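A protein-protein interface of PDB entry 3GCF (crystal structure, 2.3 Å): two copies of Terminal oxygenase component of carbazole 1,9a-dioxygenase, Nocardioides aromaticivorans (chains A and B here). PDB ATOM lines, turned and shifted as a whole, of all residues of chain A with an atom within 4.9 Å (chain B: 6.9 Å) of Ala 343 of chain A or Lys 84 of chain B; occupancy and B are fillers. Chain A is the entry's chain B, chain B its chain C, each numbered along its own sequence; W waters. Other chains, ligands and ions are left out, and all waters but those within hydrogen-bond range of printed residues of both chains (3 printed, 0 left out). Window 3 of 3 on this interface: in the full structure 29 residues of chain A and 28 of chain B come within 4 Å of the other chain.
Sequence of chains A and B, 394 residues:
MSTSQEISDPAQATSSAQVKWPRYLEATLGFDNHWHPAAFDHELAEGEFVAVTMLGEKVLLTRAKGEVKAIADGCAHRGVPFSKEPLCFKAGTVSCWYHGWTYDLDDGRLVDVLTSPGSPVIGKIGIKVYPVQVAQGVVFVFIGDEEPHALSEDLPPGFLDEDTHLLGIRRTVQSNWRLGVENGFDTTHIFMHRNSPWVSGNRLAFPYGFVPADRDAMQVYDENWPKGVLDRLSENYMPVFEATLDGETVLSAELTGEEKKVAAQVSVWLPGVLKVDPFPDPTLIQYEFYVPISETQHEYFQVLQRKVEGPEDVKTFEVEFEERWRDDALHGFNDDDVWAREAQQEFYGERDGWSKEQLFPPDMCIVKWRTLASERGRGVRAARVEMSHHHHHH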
ATOM      1  N   TRP A 339      16.087  23.230   5.898  1.00  0.00           N
ATOM      2  CA  TRP A 339      15.200  23.280   4.737  1.00  0.00           C
ATOM      3  C   TRP A 339      15.263  21.999   3.913  1.00  0.00           C
ATOM      4  O   TRP A 339      14.317  21.675   3.198  1.00  0.00           O
ATOM      5  CB  TRP A 339      15.461  24.513   3.842  1.00  0.00           C
ATOM      6  CG  TRP A 339      16.842  24.664   3.242  1.00  0.00           C
ATOM      7  CD1 TRP A 339      17.862  25.429   3.725  1.00  0.00           C
ATOM      8  CD2 TRP A 339      17.322  24.081   2.020  1.00  0.00           C
ATOM      9  NE1 TRP A 339      18.948  25.362   2.883  1.00  0.00           N
ATOM     10  CE2 TRP A 339      18.646  24.542   1.830  1.00  0.00           C
ATOM     11  CE3 TRP A 339      16.764  23.216   1.068  1.00  0.00           C
ATOM     12  CZ2 TRP A 339      19.424  24.167   0.723  1.00  0.00           C
ATOM     13  CZ3 TRP A 339      17.539  22.841  -0.036  1.00  0.00           C
ATOM     14  CH2 TRP A 339      18.857  23.320  -0.195  1.00  0.00           C
ATOM     15  N   ALA A 340      16.363  21.259   4.022  1.00  0.00           N
ATOM     16  CA  ALA A 340      16.484  20.003   3.286  1.00  0.00           C
ATOM     17  C   ALA A 340      15.452  19.016   3.818  1.00  0.00           C
ATOM     18  O   ALA A 340      14.847  18.265   3.055  1.00  0.00           O
ATOM     19  CB  ALA A 340      17.886  19.423   3.443  1.00  0.00           C
ATOM     20  N   ARG A 341      15.264  19.011   5.132  1.00  0.00           N
ATOM     21  CA  ARG A 341      14.294  18.121   5.755  1.00  0.00           C
ATOM     22  C   ARG A 341      12.886  18.539   5.362  1.00  0.00           C
ATOM     23  O   ARG A 341      12.068  17.713   4.961  1.00  0.00           O
ATOM     24  CB  ARG A 341      14.430  18.170   7.280  1.00  0.00           C
ATOM     25  CG  ARG A 341      15.753  17.638   7.797  1.00  0.00           C
ATOM     26  CD  ARG A 341      15.925  17.882   9.288  1.00  0.00           C
ATOM     27  NE  ARG A 341      17.312  17.653   9.681  1.00  0.00           N
ATOM     28  CZ  ARG A 341      17.819  17.921  10.879  1.00  0.00           C
ATOM     29  NH1 ARG A 341      17.057  18.431  11.836  1.00  0.00           N
ATOM     30  NH2 ARG A 341      19.106  17.702  11.107  1.00  0.00           N
ATOM     31  N   GLU A 342      12.614  19.834   5.472  1.00  0.00           N
ATOM     32  CA  GLU A 342      11.295  20.370   5.149  1.00  0.00           C
ATOM     33  C   GLU A 342      10.928  20.199   3.679  1.00  0.00           C
ATOM     34  O   GLU A 342       9.751  20.145   3.332  1.00  0.00           O
ATOM     35  CB  GLU A 342      11.230  21.845   5.561  1.00  0.00           C
ATOM     36  CG  GLU A 342      11.629  22.046   7.016  1.00  0.00           C
ATOM     37  CD  GLU A 342      11.698  23.502   7.436  1.00  0.00           C
ATOM     38  OE1 GLU A 342      12.065  24.359   6.603  1.00  0.00           O
ATOM     39  OE2 GLU A 342      11.405  23.789   8.613  1.00  0.00           O
ATOM     40  N   ALA A 343      11.933  20.104   2.814  1.00  0.00           N
ATOM     41  CA  ALA A 343      11.684  19.924   1.386  1.00  0.00           C
ATOM     42  C   ALA A 343      11.138  18.519   1.106  1.00  0.00           C
ATOM     43  O   ALA A 343      10.587  18.260   0.037  1.00  0.00           O
ATOM     44  CB  ALA A 343      12.971  20.148   0.602  1.00  0.00           C
ATOM     45  N   GLN A 344      11.289  17.623   2.079  1.00  0.00           N
ATOM     46  CA  GLN A 344      10.830  16.240   1.951  1.00  0.00           C
ATOM     47  C   GLN A 344       9.462  16.009   2.600  1.00  0.00           C
ATOM     48  O   GLN A 344       8.801  15.006   2.327  1.00  0.00           O
ATOM     49  CB  GLN A 344      11.843  15.282   2.610  1.00  0.00           C
ATOM     50  CG  GLN A 344      13.258  15.325   2.039  1.00  0.00           C
ATOM     51  CD  GLN A 344      14.271  14.545   2.887  1.00  0.00           C
ATOM     52  OE1 GLN A 344      14.193  13.325   3.008  1.00  0.00           O
ATOM     53  NE2 GLN A 344      15.222  15.260   3.479  1.00  0.00           N
ATOM     54  N   GLN A 345       9.049  16.932   3.462  1.00  0.00           N
ATOM     55  CA  GLN A 345       7.790  16.808   4.195  1.00  0.00           C
ATOM     56  C   GLN A 345       6.556  16.471   3.359  1.00  0.00           C
ATOM     57  O   GLN A 345       5.814  15.549   3.692  1.00  0.00           O
ATOM     58  CB  GLN A 345       7.540  18.082   5.011  1.00  0.00           C
ATOM     59  CG  GLN A 345       6.297  18.036   5.893  1.00  0.00           C
ATOM     60  CD  GLN A 345       6.225  16.784   6.749  1.00  0.00           C
ATOM     61  OE1 GLN A 345       7.248  16.267   7.208  1.00  0.00           O
ATOM     62  NE2 GLN A 345       5.009  16.299   6.985  1.00  0.00           N
ATOM     63  N   LYS B  58       3.978  19.554 -10.482  1.00  0.00           N
ATOM     64  CA  LYS B  58       5.064  20.520 -10.374  1.00  0.00           C
ATOM     65  C   LYS B  58       6.027  20.238 -11.518  1.00  0.00           C
ATOM     66  O   LYS B  58       6.510  19.120 -11.673  1.00  0.00           O
ATOM     67  CB  LYS B  58       5.780  20.388  -9.027  1.00  0.00           C
ATOM     68  CG  LYS B  58       4.892  20.690  -7.831  1.00  0.00           C
ATOM     69  CD  LYS B  58       5.710  20.926  -6.568  1.00  0.00           C
ATOM     70  CE  LYS B  58       6.589  22.166  -6.702  1.00  0.00           C
ATOM     71  NZ  LYS B  58       7.300  22.519  -5.438  1.00  0.00           N
ATOM     72  N   LEU B  60       9.486  21.695 -13.867  1.00  0.00           N
ATOM     73  CA  LEU B  60      10.662  22.557 -13.874  1.00  0.00           C
ATOM     74  C   LEU B  60      11.017  22.846 -15.323  1.00  0.00           C
ATOM     75  O   LEU B  60      11.196  21.921 -16.120  1.00  0.00           O
ATOM     76  CB  LEU B  60      11.853  21.868 -13.199  1.00  0.00           C
ATOM     77  CG  LEU B  60      13.145  22.692 -13.129  1.00  0.00           C
ATOM     78  CD1 LEU B  60      12.967  23.822 -12.125  1.00  0.00           C
ATOM     79  CD2 LEU B  60      14.311  21.808 -12.709  1.00  0.00           C
ATOM     80  N   ASP B  73       9.398  18.342 -11.510  1.00  0.00           N
ATOM     81  CA  ASP B  73      10.131  19.029 -10.453  1.00  0.00           C
ATOM     82  C   ASP B  73      10.055  18.197  -9.175  1.00  0.00           C
ATOM     83  O   ASP B  73       9.502  18.625  -8.153  1.00  0.00           O
ATOM     84  CB  ASP B  73       9.528  20.418 -10.232  1.00  0.00           C
ATOM     85  CG  ASP B  73      10.328  21.257  -9.261  1.00  0.00           C
ATOM     86  OD1 ASP B  73      11.517  20.945  -9.028  1.00  0.00           O
ATOM     87  OD2 ASP B  73       9.768  22.247  -8.742  1.00  0.00           O
ATOM     88  N   ARG B  78      14.398  10.888  -3.119  1.00  0.00           N
ATOM     89  CA  ARG B  78      13.578  11.152  -1.946  1.00  0.00           C
ATOM     90  C   ARG B  78      12.497  12.196  -2.215  1.00  0.00           C
ATOM     91  O   ARG B  78      12.019  12.869  -1.303  1.00  0.00           O
ATOM     92  CB  ARG B  78      14.462  11.564  -0.765  1.00  0.00           C
ATOM     93  CG  ARG B  78      15.451  10.471  -0.337  1.00  0.00           C
ATOM     94  CD  ARG B  78      16.134  10.837   0.976  1.00  0.00           C
ATOM     95  NE  ARG B  78      15.169  10.887   2.073  1.00  0.00           N
ATOM     96  CZ  ARG B  78      15.115  10.004   3.064  1.00  0.00           C
ATOM     97  NH1 ARG B  78      15.981   8.995   3.112  1.00  0.00           N
ATOM     98  NH2 ARG B  78      14.181  10.117   4.000  1.00  0.00           N
ATOM     99  N   GLY B  79      12.136  12.330  -3.486  1.00  0.00           N
ATOM    100  CA  GLY B  79      11.071  13.233  -3.886  1.00  0.00           C
ATOM    101  C   GLY B  79      11.186  14.738  -3.763  1.00  0.00           C
ATOM    102  O   GLY B  79      10.210  15.428  -4.043  1.00  0.00           O
ATOM    103  N   VAL B  80      12.338  15.268  -3.364  1.00  0.00           N
ATOM    104  CA  VAL B  80      12.450  16.719  -3.238  1.00  0.00           C
ATOM    105  C   VAL B  80      12.368  17.425  -4.587  1.00  0.00           C
ATOM    106  O   VAL B  80      12.695  16.851  -5.627  1.00  0.00           O
ATOM    107  CB  VAL B  80      13.774  17.152  -2.550  1.00  0.00           C
ATOM    108  CG1 VAL B  80      13.912  16.464  -1.195  1.00  0.00           C
ATOM    109  CG2 VAL B  80      14.968  16.841  -3.455  1.00  0.00           C
ATOM    110  N   PRO B  81      11.882  18.673  -4.593  1.00  0.00           N
ATOM    111  CA  PRO B  81      11.792  19.413  -5.856  1.00  0.00           C
ATOM    112  C   PRO B  81      13.146  20.040  -6.169  1.00  0.00           C
ATOM    113  O   PRO B  81      13.816  20.547  -5.269  1.00  0.00           O
ATOM    114  CB  PRO B  81      10.715  20.462  -5.573  1.00  0.00           C
ATOM    115  CG  PRO B  81      10.836  20.690  -4.092  1.00  0.00           C
ATOM    116  CD  PRO B  81      11.039  19.294  -3.551  1.00  0.00           C
ATOM    117  N   PHE B  82      13.556  19.994  -7.435  1.00  0.00           N
ATOM    118  CA  PHE B  82      14.836  20.573  -7.830  1.00  0.00           C
ATOM    119  C   PHE B  82      14.783  22.083  -7.644  1.00  0.00           C
ATOM    120  O   PHE B  82      15.800  22.714  -7.334  1.00  0.00           O
ATOM    121  CB  PHE B  82      15.144  20.278  -9.306  1.00  0.00           C
ATOM    122  CG  PHE B  82      15.053  18.825  -9.674  1.00  0.00           C
ATOM    123  CD1 PHE B  82      15.833  17.875  -9.025  1.00  0.00           C
ATOM    124  CD2 PHE B  82      14.193  18.407 -10.681  1.00  0.00           C
ATOM    125  CE1 PHE B  82      15.757  16.527  -9.371  1.00  0.00           C
ATOM    126  CE2 PHE B  82      14.109  17.062 -11.035  1.00  0.00           C
ATOM    127  CZ  PHE B  82      14.894  16.121 -10.377  1.00  0.00           C
ATOM    128  N   SER B  83      13.596  22.657  -7.841  1.00  0.00           N
ATOM    129  CA  SER B  83      13.415  24.099  -7.728  1.00  0.00           C
ATOM    130  C   SER B  83      13.876  24.685  -6.392  1.00  0.00           C
ATOM    131  O   SER B  83      14.133  25.880  -6.300  1.00  0.00           O
ATOM    132  CB  SER B  83      11.955  24.491  -8.028  1.00  0.00           C
ATOM    133  OG  SER B  83      11.031  23.792  -7.221  1.00  0.00           O
ATOM    134  N   LYS B  84      13.992  23.855  -5.358  1.00  0.00           N
ATOM    135  CA  LYS B  84      14.488  24.355  -4.077  1.00  0.00           C
ATOM    136  C   LYS B  84      15.885  24.936  -4.292  1.00  0.00           C
ATOM    137  O   LYS B  84      16.260  25.917  -3.660  1.00  0.00           O
ATOM    138  CB  LYS B  84      14.566  23.232  -3.029  1.00  0.00           C
ATOM    139  CG  LYS B  84      13.246  22.961  -2.325  1.00  0.00           C
ATOM    140  CD  LYS B  84      12.791  24.198  -1.546  1.00  0.00           C
ATOM    141  CE  LYS B  84      11.313  24.125  -1.164  1.00  0.00           C
ATOM    142  NZ  LYS B  84      10.992  23.004  -0.237  1.00  0.00           N
ATOM    143  N   GLU B  85      16.648  24.320  -5.194  1.00  0.00           N
ATOM    144  CA  GLU B  85      18.007  24.762  -5.503  1.00  0.00           C
ATOM    145  C   GLU B  85      18.407  24.043  -6.788  1.00  0.00           C
ATOM    146  O   GLU B  85      19.158  23.065  -6.767  1.00  0.00           O
ATOM    147  CB  GLU B  85      18.954  24.388  -4.358  1.00  0.00           C
ATOM    148  CG  GLU B  85      20.401  24.834  -4.557  1.00  0.00           C
ATOM    149  CD  GLU B  85      21.266  24.573  -3.331  1.00  0.00           C
ATOM    150  OE1 GLU B  85      21.181  25.347  -2.355  1.00  0.00           O
ATOM    151  OE2 GLU B  85      22.026  23.584  -3.339  1.00  0.00           O
ATOM    152  N   PRO B  86      17.891  24.521  -7.930  1.00  0.00           N
ATOM    153  CA  PRO B  86      18.166  23.936  -9.245  1.00  0.00           C
ATOM    154  C   PRO B  86      19.631  23.990  -9.650  1.00  0.00           C
ATOM    155  O   PRO B  86      20.260  25.042  -9.601  1.00  0.00           O
ATOM    156  CB  PRO B  86      17.256  24.740 -10.173  1.00  0.00           C
ATOM    157  CG  PRO B  86      17.236  26.091  -9.517  1.00  0.00           C
ATOM    158  CD  PRO B  86      17.079  25.748  -8.057  1.00  0.00           C
ATOM    159  N   TRP B  97      19.969  18.807  -5.916  1.00  0.00           N
ATOM    160  CA  TRP B  97      20.812  19.472  -4.936  1.00  0.00           C
ATOM    161  C   TRP B  97      21.092  18.629  -3.695  1.00  0.00           C
ATOM    162  O   TRP B  97      21.989  18.950  -2.912  1.00  0.00           O
ATOM    163  CB  TRP B  97      20.148  20.773  -4.478  1.00  0.00           C
ATOM    164  CG  TRP B  97      18.725  20.572  -3.996  1.00  0.00           C
ATOM    165  CD1 TRP B  97      17.580  20.695  -4.738  1.00  0.00           C
ATOM    166  CD2 TRP B  97      18.309  20.151  -2.689  1.00  0.00           C
ATOM    167  NE1 TRP B  97      16.478  20.376  -3.972  1.00  0.00           N
ATOM    168  CE2 TRP B  97      16.896  20.038  -2.713  1.00  0.00           C
ATOM    169  CE3 TRP B  97      18.991  19.854  -1.500  1.00  0.00           C
ATOM    170  CZ2 TRP B  97      16.154  19.641  -1.590  1.00  0.00           C
ATOM    171  CZ3 TRP B  97      18.252  19.456  -0.384  1.00  0.00           C
ATOM    172  CH2 TRP B  97      16.849  19.354  -0.439  1.00  0.00           C
HETATM  173  O   HOH W   1      12.302  23.555   2.051  1.00  0.00           O
HETATM  174  O   HOH W   2      15.750  12.810   5.244  1.00  0.00           O
HETATM  175  O   HOH W   3       9.464  23.021   1.830  1.00  0.00           O
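NE of Arg 78 of chain B is in hydrogen-bond range of OE1 of Gln 344 of chain A, 2.8 Å away.
The backbone carbonyl oxygen of Ala 340 of chain A sits at hydrogen-bond distance from the side-chain amide nitrogen of Gln 344 of chain A, at 3.1 Å.
The indole nitrogen (NE1) of Trp 97 of chain B lies within hydrogen-bond range of the backbone carbonyl oxygen (O) of Pro 81 of chain B, at 3.0 Å.
Among the printed residues, pairs that only touch across the chains: Trp 339 of chain A with Trp 97 of chain B (3.5 Å), Gln 344 of chain A with Val 80 of chain B (3.5 Å), Ala 343 of chain A with Lys 84 of chain B (3.5 Å), Trp 339 of chain A with Glu 85 of chain B (3.7 Å), Ala 343 of chain A with Pro 81 of chain B (3.8 Å), Ala 340 of chain A with Trp 97 of chain B (3.8 Å), Ala 343 of chain A with Trp 97 of chain B (3.9 Å) and Ala 343 of chain A with Val 80 of chain B (3.97 Å).
Printed residues of chain B within 4 Å of Ala 343 of chain A: Val 80 (3.97 Å), Pro 81 (3.8 Å), Lys 84 (3.5 Å) and Trp 97 (3.9 Å).
Printed residues of chain B within 4 Å of Gln 344 of chain A: Arg 78 and Val 80.
Printed residues of chain A within 4 Å of Arg 78 of chain B: Gln 344 (2.8 Å).
Gly 79 of chain B touches none of the printed residues of chain A.
Printed residues of chain A within 4 Å of Lys 84 of chain B: Ala 343 (3.5 Å).
Printed residues of chain A within 4 Å of Glu 85 of chain B: Trp 339 (3.7 Å).
Of the 7 printed residues of chain A, 4 touch a printed residue of chain B.
Printed residues of chain A that touch a printed residue of chain B: Trp 339, Ala 340, Ala 343 and Gln 344.
Hydrophobic or aromatic side chains of chain A that line the printed part of chain B: Trp 339, Ala 340 and Ala 343.
Of the 13 printed residues of chain B, 6 touch a printed residue of chain A.
Printed residues of chain B that touch a printed residue of chain A: Arg 78, Val 80, Pro 81, Lys 84, Glu 85 and Trp 97.
Hydrophobic or aromatic side chains of chain B that line the printed part of chain A: Val 80, Pro 81 and Trp 97.
No position is printed for both chains.
Of the 9 pairs that touch across the chains among the printed residues, none has its exchanged pair printed and touching as well.
Water W3 lies within hydrogen-bond range of NZ of Lys 84 of chain B (2.6 Å) and O of Glu 342 of chain A (3.3 Å).
Water W1 bridges the side-chain amino group of Lys 84 of chain B (2.7 Å) and the backbone carbonyl oxygen of Trp 339 of chain A (3.0 Å).
Water W2 bridges the side-chain amide oxygen (OE1) of Gln 344 of chain A (2.8 Å) and the guanidinium group (NH2) of Arg 78 of chain B (3.4 Å).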
